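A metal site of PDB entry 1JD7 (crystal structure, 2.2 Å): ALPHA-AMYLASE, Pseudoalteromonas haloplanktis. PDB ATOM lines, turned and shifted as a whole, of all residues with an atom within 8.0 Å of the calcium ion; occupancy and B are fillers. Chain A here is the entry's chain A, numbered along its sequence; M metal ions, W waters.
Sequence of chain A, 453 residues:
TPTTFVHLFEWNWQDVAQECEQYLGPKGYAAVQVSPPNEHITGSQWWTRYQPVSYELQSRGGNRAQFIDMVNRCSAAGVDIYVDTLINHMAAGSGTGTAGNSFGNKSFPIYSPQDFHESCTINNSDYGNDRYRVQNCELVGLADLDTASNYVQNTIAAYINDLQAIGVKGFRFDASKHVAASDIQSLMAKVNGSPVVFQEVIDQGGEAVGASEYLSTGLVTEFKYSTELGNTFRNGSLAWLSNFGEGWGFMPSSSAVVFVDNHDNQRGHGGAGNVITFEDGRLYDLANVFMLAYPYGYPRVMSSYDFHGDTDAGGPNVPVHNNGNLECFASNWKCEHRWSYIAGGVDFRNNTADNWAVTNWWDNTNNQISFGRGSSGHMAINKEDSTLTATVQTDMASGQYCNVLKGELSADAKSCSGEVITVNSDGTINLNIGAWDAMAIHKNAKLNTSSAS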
ATOM      1  N   ILE A  87     -16.286 -27.061 -22.357  1.00  0.00           N
ATOM      2  CA  ILE A  87     -16.561 -27.068 -23.794  1.00  0.00           C
ATOM      3  C   ILE A  87     -15.697 -26.132 -24.636  1.00  0.00           C
ATOM      4  O   ILE A  87     -15.800 -26.127 -25.864  1.00  0.00           O
ATOM      5  CB  ILE A  87     -18.021 -26.708 -24.078  1.00  0.00           C
ATOM      6  CG1 ILE A  87     -18.240 -25.220 -23.775  1.00  0.00           C
ATOM      7  CG2 ILE A  87     -18.947 -27.543 -23.216  1.00  0.00           C
ATOM      8  CD1 ILE A  87     -19.505 -24.662 -24.325  1.00  0.00           C
ATOM      9  N   ASN A  88     -14.843 -25.336 -23.984  1.00  0.00           N
ATOM     10  CA  ASN A  88     -14.032 -24.354 -24.699  1.00  0.00           C
ATOM     11  C   ASN A  88     -12.558 -24.659 -24.913  1.00  0.00           C
ATOM     12  O   ASN A  88     -11.962 -24.179 -25.880  1.00  0.00           O
ATOM     13  CB  ASN A  88     -14.148 -23.001 -23.992  1.00  0.00           C
ATOM     14  CG  ASN A  88     -13.291 -21.919 -24.636  1.00  0.00           C
ATOM     15  OD1 ASN A  88     -13.620 -21.410 -25.714  1.00  0.00           O
ATOM     16  ND2 ASN A  88     -12.196 -21.550 -23.982  1.00  0.00           N
ATOM     17  N   HIS A  89     -11.951 -25.468 -24.052  1.00  0.00           N
ATOM     18  CA  HIS A  89     -10.520 -25.695 -24.180  1.00  0.00           C
ATOM     19  C   HIS A  89      -9.965 -26.972 -23.559  1.00  0.00           C
ATOM     20  O   HIS A  89     -10.687 -27.751 -22.935  1.00  0.00           O
ATOM     21  CB  HIS A  89      -9.803 -24.517 -23.529  1.00  0.00           C
ATOM     22  CG  HIS A  89     -10.270 -24.269 -22.129  1.00  0.00           C
ATOM     23  ND1 HIS A  89     -11.335 -23.441 -21.817  1.00  0.00           N
ATOM     24  CD2 HIS A  89      -9.883 -24.814 -20.948  1.00  0.00           C
ATOM     25  CE1 HIS A  89     -11.580 -23.487 -20.520  1.00  0.00           C
ATOM     26  NE2 HIS A  89     -10.710 -24.311 -19.969  1.00  0.00           N
ATOM     27  N   HIS A 117      -7.913 -24.033 -32.443  1.00  0.00           N
ATOM     28  CA  HIS A 117      -7.860 -22.783 -33.166  1.00  0.00           C
ATOM     29  C   HIS A 117      -6.391 -22.381 -33.129  1.00  0.00           C
ATOM     30  O   HIS A 117      -5.680 -22.689 -32.164  1.00  0.00           O
ATOM     31  CB  HIS A 117      -8.684 -21.721 -32.441  1.00  0.00           C
ATOM     32  CG  HIS A 117     -10.165 -21.860 -32.620  1.00  0.00           C
ATOM     33  ND1 HIS A 117     -11.067 -21.397 -31.685  1.00  0.00           N
ATOM     34  CD2 HIS A 117     -10.895 -22.351 -33.646  1.00  0.00           C
ATOM     35  CE1 HIS A 117     -12.287 -21.586 -32.136  1.00  0.00           C
ATOM     36  NE2 HIS A 117     -12.215 -22.168 -33.316  1.00  0.00           N
ATOM     37  N   ILE A 122      -5.972 -13.838 -25.779  1.00  0.00           N
ATOM     38  CA  ILE A 122      -7.111 -12.954 -25.569  1.00  0.00           C
ATOM     39  C   ILE A 122      -6.638 -11.799 -24.704  1.00  0.00           C
ATOM     40  O   ILE A 122      -6.134 -12.011 -23.606  1.00  0.00           O
ATOM     41  CB  ILE A 122      -8.255 -13.652 -24.843  1.00  0.00           C
ATOM     42  CG1 ILE A 122      -8.808 -14.788 -25.703  1.00  0.00           C
ATOM     43  CG2 ILE A 122      -9.326 -12.641 -24.500  1.00  0.00           C
ATOM     44  CD1 ILE A 122      -9.907 -15.552 -25.023  1.00  0.00           C
ATOM     45  N   TYR A 132     -14.317 -11.963 -32.306  1.00  0.00           N
ATOM     46  CA  TYR A 132     -13.484 -12.997 -32.897  1.00  0.00           C
ATOM     47  C   TYR A 132     -12.380 -13.495 -31.980  1.00  0.00           C
ATOM     48  O   TYR A 132     -12.248 -14.695 -31.745  1.00  0.00           O
ATOM     49  CB  TYR A 132     -12.865 -12.520 -34.209  1.00  0.00           C
ATOM     50  CG  TYR A 132     -12.071 -13.593 -34.916  1.00  0.00           C
ATOM     51  CD1 TYR A 132     -12.713 -14.558 -35.687  1.00  0.00           C
ATOM     52  CD2 TYR A 132     -10.691 -13.690 -34.746  1.00  0.00           C
ATOM     53  CE1 TYR A 132     -12.001 -15.603 -36.277  1.00  0.00           C
ATOM     54  CE2 TYR A 132      -9.966 -14.730 -35.334  1.00  0.00           C
ATOM     55  CZ  TYR A 132     -10.623 -15.681 -36.096  1.00  0.00           C
ATOM     56  OH  TYR A 132      -9.915 -16.726 -36.662  1.00  0.00           O
ATOM     57  N   ARG A 133     -11.566 -12.577 -31.462  1.00  0.00           N
ATOM     58  CA  ARG A 133     -10.461 -12.965 -30.584  1.00  0.00           C
ATOM     59  C   ARG A 133     -10.943 -13.567 -29.264  1.00  0.00           C
ATOM     60  O   ARG A 133     -10.285 -14.432 -28.701  1.00  0.00           O
ATOM     61  CB  ARG A 133      -9.552 -11.773 -30.302  1.00  0.00           C
ATOM     62  CG  ARG A 133      -8.729 -11.311 -31.507  1.00  0.00           C
ATOM     63  CD  ARG A 133      -7.836 -10.148 -31.124  1.00  0.00           C
ATOM     64  NE  ARG A 133      -6.749 -10.541 -30.224  1.00  0.00           N
ATOM     65  CZ  ARG A 133      -5.645 -11.162 -30.622  1.00  0.00           C
ATOM     66  NH1 ARG A 133      -4.704 -11.491 -29.744  1.00  0.00           N
ATOM     67  NH2 ARG A 133      -5.475 -11.463 -31.906  1.00  0.00           N
ATOM     68  N   VAL A 134     -12.095 -13.120 -28.770  1.00  0.00           N
ATOM     69  CA  VAL A 134     -12.645 -13.637 -27.523  1.00  0.00           C
ATOM     70  C   VAL A 134     -13.025 -15.120 -27.654  1.00  0.00           C
ATOM     71  O   VAL A 134     -12.790 -15.906 -26.731  1.00  0.00           O
ATOM     72  CB  VAL A 134     -13.902 -12.811 -27.070  1.00  0.00           C
ATOM     73  CG1 VAL A 134     -14.688 -13.558 -25.997  1.00  0.00           C
ATOM     74  CG2 VAL A 134     -13.477 -11.448 -26.520  1.00  0.00           C
ATOM     75  N   GLN A 135     -13.584 -15.511 -28.804  1.00  0.00           N
ATOM     76  CA  GLN A 135     -14.016 -16.885 -29.018  1.00  0.00           C
ATOM     77  C   GLN A 135     -13.039 -17.755 -29.823  1.00  0.00           C
ATOM     78  O   GLN A 135     -13.255 -18.949 -29.973  1.00  0.00           O
ATOM     79  CB  GLN A 135     -15.409 -16.894 -29.689  1.00  0.00           C
ATOM     80  CG  GLN A 135     -16.405 -15.971 -28.980  1.00  0.00           C
ATOM     81  CD  GLN A 135     -17.791 -15.961 -29.603  1.00  0.00           C
ATOM     82  OE1 GLN A 135     -17.932 -15.977 -30.831  1.00  0.00           O
ATOM     83  NE2 GLN A 135     -18.822 -15.909 -28.761  1.00  0.00           N
ATOM     84  N   ASN A 136     -11.962 -17.163 -30.302  1.00  0.00           N
ATOM     85  CA  ASN A 136     -11.001 -17.931 -31.078  1.00  0.00           C
ATOM     86  C   ASN A 136      -9.598 -17.968 -30.484  1.00  0.00           C
ATOM     87  O   ASN A 136      -8.821 -18.864 -30.808  1.00  0.00           O
ATOM     88  CB  ASN A 136     -10.957 -17.422 -32.510  1.00  0.00           C
ATOM     89  CG  ASN A 136     -12.224 -17.744 -33.265  1.00  0.00           C
ATOM     90  OD1 ASN A 136     -12.452 -18.889 -33.656  1.00  0.00           O
ATOM     91  ND2 ASN A 136     -13.080 -16.743 -33.436  1.00  0.00           N
ATOM     92  N   CYS A 137      -9.277 -17.000 -29.632  1.00  0.00           N
ATOM     93  CA  CYS A 137      -7.966 -16.984 -28.998  1.00  0.00           C
ATOM     94  C   CYS A 137      -8.012 -17.662 -27.636  1.00  0.00           C
ATOM     95  O   CYS A 137      -9.086 -17.917 -27.100  1.00  0.00           O
ATOM     96  CB  CYS A 137      -7.426 -15.562 -28.880  1.00  0.00           C
ATOM     97  SG  CYS A 137      -7.116 -14.808 -30.519  1.00  0.00           S
ATOM     98  N   GLU A 138      -6.844 -17.940 -27.071  1.00  0.00           N
ATOM     99  CA  GLU A 138      -6.741 -18.648 -25.808  1.00  0.00           C
ATOM    100  C   GLU A 138      -7.054 -17.879 -24.519  1.00  0.00           C
ATOM    101  O   GLU A 138      -6.648 -16.730 -24.326  1.00  0.00           O
ATOM    102  CB  GLU A 138      -5.348 -19.283 -25.703  1.00  0.00           C
ATOM    103  CG  GLU A 138      -4.887 -19.931 -27.009  1.00  0.00           C
ATOM    104  CD  GLU A 138      -3.473 -20.512 -26.966  1.00  0.00           C
ATOM    105  OE1 GLU A 138      -2.517 -19.788 -26.601  1.00  0.00           O
ATOM    106  OE2 GLU A 138      -3.310 -21.696 -27.324  1.00  0.00           O
ATOM    107  N   LEU A 139      -7.817 -18.534 -23.639  1.00  0.00           N
ATOM    108  CA  LEU A 139      -8.158 -17.982 -22.342  1.00  0.00           C
ATOM    109  C   LEU A 139      -7.039 -18.447 -21.406  1.00  0.00           C
ATOM    110  O   LEU A 139      -6.885 -19.650 -21.161  1.00  0.00           O
ATOM    111  CB  LEU A 139      -9.504 -18.545 -21.862  1.00  0.00           C
ATOM    112  CG  LEU A 139      -9.896 -18.214 -20.428  1.00  0.00           C
ATOM    113  CD1 LEU A 139     -10.101 -16.708 -20.268  1.00  0.00           C
ATOM    114  CD2 LEU A 139     -11.155 -18.965 -20.071  1.00  0.00           C
ATOM    115  N   LEU A 142      -4.887 -21.400 -22.450  1.00  0.00           N
ATOM    116  CA  LEU A 142      -5.479 -22.729 -22.625  1.00  0.00           C
ATOM    117  C   LEU A 142      -5.771 -23.023 -24.110  1.00  0.00           C
ATOM    118  O   LEU A 142      -6.359 -22.172 -24.805  1.00  0.00           O
ATOM    119  CB  LEU A 142      -6.763 -22.843 -21.799  1.00  0.00           C
ATOM    120  CG  LEU A 142      -6.632 -22.592 -20.272  1.00  0.00           C
ATOM    121  CD1 LEU A 142      -8.012 -22.505 -19.633  1.00  0.00           C
ATOM    122  CD2 LEU A 142      -5.810 -23.697 -19.632  1.00  0.00           C
ATOM    123  N   ALA A 143      -5.378 -24.194 -24.592  1.00  0.00           N
ATOM    124  CA  ALA A 143      -5.590 -24.567 -26.002  1.00  0.00           C
ATOM    125  C   ALA A 143      -7.065 -24.408 -26.374  1.00  0.00           C
ATOM    126  O   ALA A 143      -7.920 -25.160 -25.890  1.00  0.00           O
ATOM    127  CB  ALA A 143      -5.143 -26.019 -26.238  1.00  0.00           C
ATOM    128  N   ASP A 144      -7.353 -23.446 -27.243  1.00  0.00           N
ATOM    129  CA  ASP A 144      -8.735 -23.170 -27.630  1.00  0.00           C
ATOM    130  C   ASP A 144      -9.273 -24.113 -28.701  1.00  0.00           C
ATOM    131  O   ASP A 144      -8.919 -24.012 -29.876  1.00  0.00           O
ATOM    132  CB  ASP A 144      -8.836 -21.714 -28.087  1.00  0.00           C
ATOM    133  CG  ASP A 144     -10.254 -21.188 -28.034  1.00  0.00           C
ATOM    134  OD1 ASP A 144     -10.827 -21.108 -26.921  1.00  0.00           O
ATOM    135  OD2 ASP A 144     -10.791 -20.851 -29.110  1.00  0.00           O
ATOM    136  N   LEU A 145     -10.128 -25.039 -28.278  1.00  0.00           N
ATOM    137  CA  LEU A 145     -10.734 -26.031 -29.175  1.00  0.00           C
ATOM    138  C   LEU A 145     -11.508 -25.377 -30.322  1.00  0.00           C
ATOM    139  O   LEU A 145     -12.096 -24.314 -30.165  1.00  0.00           O
ATOM    140  CB  LEU A 145     -11.680 -26.949 -28.388  1.00  0.00           C
ATOM    141  CG  LEU A 145     -11.119 -28.082 -27.512  1.00  0.00           C
ATOM    142  CD1 LEU A 145     -12.194 -28.555 -26.546  1.00  0.00           C
ATOM    143  CD2 LEU A 145     -10.646 -29.237 -28.391  1.00  0.00           C
ATOM    144  N   ASP A 146     -11.491 -26.023 -31.480  1.00  0.00           N
ATOM    145  CA  ASP A 146     -12.221 -25.513 -32.625  1.00  0.00           C
ATOM    146  C   ASP A 146     -13.638 -26.056 -32.506  1.00  0.00           C
ATOM    147  O   ASP A 146     -13.998 -27.062 -33.120  1.00  0.00           O
ATOM    148  CB  ASP A 146     -11.561 -25.988 -33.930  1.00  0.00           C
ATOM    149  CG  ASP A 146     -12.305 -25.529 -35.165  1.00  0.00           C
ATOM    150  OD1 ASP A 146     -13.140 -24.614 -35.061  1.00  0.00           O
ATOM    151  OD2 ASP A 146     -12.047 -26.096 -36.254  1.00  0.00           O
ATOM    152  N   THR A 147     -14.444 -25.373 -31.698  1.00  0.00           N
ATOM    153  CA  THR A 147     -15.821 -25.775 -31.447  1.00  0.00           C
ATOM    154  C   THR A 147     -16.736 -25.729 -32.680  1.00  0.00           C
ATOM    155  O   THR A 147     -17.930 -26.033 -32.580  1.00  0.00           O
ATOM    156  CB  THR A 147     -16.429 -24.944 -30.301  1.00  0.00           C
ATOM    157  OG1 THR A 147     -16.101 -23.560 -30.488  1.00  0.00           O
ATOM    158  CG2 THR A 147     -15.887 -25.412 -28.964  1.00  0.00           C
ATOM    159  N   ALA A 175     -16.920 -21.538 -19.471  1.00  0.00           N
ATOM    160  CA  ALA A 175     -16.397 -20.569 -20.435  1.00  0.00           C
ATOM    161  C   ALA A 175     -17.238 -20.497 -21.704  1.00  0.00           C
ATOM    162  O   ALA A 175     -16.686 -20.440 -22.801  1.00  0.00           O
ATOM    163  CB  ALA A 175     -14.955 -20.932 -20.801  1.00  0.00           C
ATOM    164  N   SER A 176     -18.563 -20.470 -21.566  1.00  0.00           N
ATOM    165  CA  SER A 176     -19.420 -20.420 -22.742  1.00  0.00           C
ATOM    166  C   SER A 176     -19.288 -19.141 -23.571  1.00  0.00           C
ATOM    167  O   SER A 176     -19.588 -19.149 -24.759  1.00  0.00           O
ATOM    168  CB  SER A 176     -20.884 -20.613 -22.343  1.00  0.00           C
ATOM    169  OG  SER A 176     -21.095 -21.938 -21.879  1.00  0.00           O
ATOM    170  N   LYS A 177     -18.849 -18.052 -22.945  1.00  0.00           N
ATOM    171  CA  LYS A 177     -18.697 -16.794 -23.670  1.00  0.00           C
ATOM    172  C   LYS A 177     -17.597 -16.917 -24.714  1.00  0.00           C
ATOM    173  O   LYS A 177     -17.633 -16.268 -25.759  1.00  0.00           O
ATOM    174  CB  LYS A 177     -18.360 -15.641 -22.704  1.00  0.00           C
ATOM    175  CG  LYS A 177     -18.048 -14.331 -23.442  1.00  0.00           C
ATOM    176  CD  LYS A 177     -18.066 -13.102 -22.535  1.00  0.00           C
ATOM    177  CE  LYS A 177     -17.015 -13.149 -21.441  1.00  0.00           C
ATOM    178  NZ  LYS A 177     -17.069 -11.910 -20.608  1.00  0.00           N
ATOM    179  N   HIS A 178     -16.623 -17.759 -24.416  1.00  0.00           N
ATOM    180  CA  HIS A 178     -15.498 -17.948 -25.326  1.00  0.00           C
ATOM    181  C   HIS A 178     -15.821 -18.915 -26.449  1.00  0.00           C
ATOM    182  O   HIS A 178     -14.951 -19.278 -27.238  1.00  0.00           O
ATOM    183  CB  HIS A 178     -14.286 -18.393 -24.513  1.00  0.00           C
ATOM    184  CG  HIS A 178     -13.868 -17.384 -23.488  1.00  0.00           C
ATOM    185  ND1 HIS A 178     -13.147 -16.259 -23.814  1.00  0.00           N
ATOM    186  CD2 HIS A 178     -14.130 -17.290 -22.163  1.00  0.00           C
ATOM    187  CE1 HIS A 178     -12.976 -15.520 -22.740  1.00  0.00           C
ATOM    188  NE2 HIS A 178     -13.563 -16.123 -21.721  1.00  0.00           N
ATOM    189  N   VAL A 179     -17.077 -19.318 -26.536  1.00  0.00           N
ATOM    190  CA  VAL A 179     -17.524 -20.228 -27.580  1.00  0.00           C
ATOM    191  C   VAL A 179     -18.750 -19.614 -28.252  1.00  0.00           C
ATOM    192  O   VAL A 179     -19.729 -19.264 -27.593  1.00  0.00           O
ATOM    193  CB  VAL A 179     -17.901 -21.617 -27.016  1.00  0.00           C
ATOM    194  CG1 VAL A 179     -18.404 -22.512 -28.130  1.00  0.00           C
ATOM    195  CG2 VAL A 179     -16.697 -22.234 -26.345  1.00  0.00           C
ATOM    196  N   ALA A 180     -18.672 -19.457 -29.574  1.00  0.00           N
ATOM    197  CA  ALA A 180     -19.767 -18.873 -30.331  1.00  0.00           C
ATOM    198  C   ALA A 180     -21.068 -19.573 -29.987  1.00  0.00           C
ATOM    199  O   ALA A 180     -21.122 -20.797 -29.872  1.00  0.00           O
ATOM    200  CB  ALA A 180     -19.487 -18.986 -31.823  1.00  0.00           C
ATOM    201  N   ASP A 183     -22.018 -22.251 -32.264  1.00  0.00           N
ATOM    202  CA  ASP A 183     -21.243 -23.477 -32.074  1.00  0.00           C
ATOM    203  C   ASP A 183     -21.930 -24.333 -30.993  1.00  0.00           C
ATOM    204  O   ASP A 183     -21.998 -25.559 -31.114  1.00  0.00           O
ATOM    205  CB  ASP A 183     -19.799 -23.173 -31.624  1.00  0.00           C
ATOM    206  CG  ASP A 183     -18.875 -22.766 -32.787  1.00  0.00           C
ATOM    207  OD1 ASP A 183     -17.683 -22.485 -32.512  1.00  0.00           O
ATOM    208  OD2 ASP A 183     -19.313 -22.715 -33.953  1.00  0.00           O
HETATM  209 CA    CA M   1     -13.051 -20.553 -27.859  1.00  0.00          CA
HETATM  210  O   HOH W   1     -13.004 -22.898 -28.035  1.00  0.00           O
HETATM  211  O   HOH W   2     -12.039 -18.454 -27.114  1.00  0.00           O
HETATM  212  O   HOH W   3     -14.497 -21.303 -29.600  1.00  0.00           O
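Water W1 lies within hydrogen-bond range of O of Leu 145 (2.7 Å) and O of Asn 88 (2.7 Å).
O of Val 134 sits at hydrogen-bond distance from ND1 of His 178.
O of Asn 88 lies within hydrogen-bond range of N of Leu 145 (3.1 Å).
The side-chain amide nitrogen (ND2) of Asn 88 lies within hydrogen-bond range of a ring nitrogen (ND1) of His 89.
The backbone carbonyl oxygen of Asp 144 lies within hydrogen-bond range of the backbone NH of His 117 (2.8 Å).
The backbone carbonyl oxygen (O) of Lys 177 is in hydrogen-bond range of the side-chain amide nitrogen (NE2) of Gln 135 (3.2 Å).
The calcium ion is bound by water W1, the backbone carbonyl oxygen (O) of His 178, the side-chain amide oxygen (OD1) of Asn 88, water W3, water W2, the side-chain carboxylate (OD1) of Asp 144, the side-chain carboxylate (OD2) of Asp 144 and the backbone carbonyl oxygen (O) of Gln 135.
Within 4 Å of the calcium ion: Asn 88, Gln 135, Asp 144 and His 178.
The nearest printed residue that does not touch the calcium ion is Val 179 (4.3 Å).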
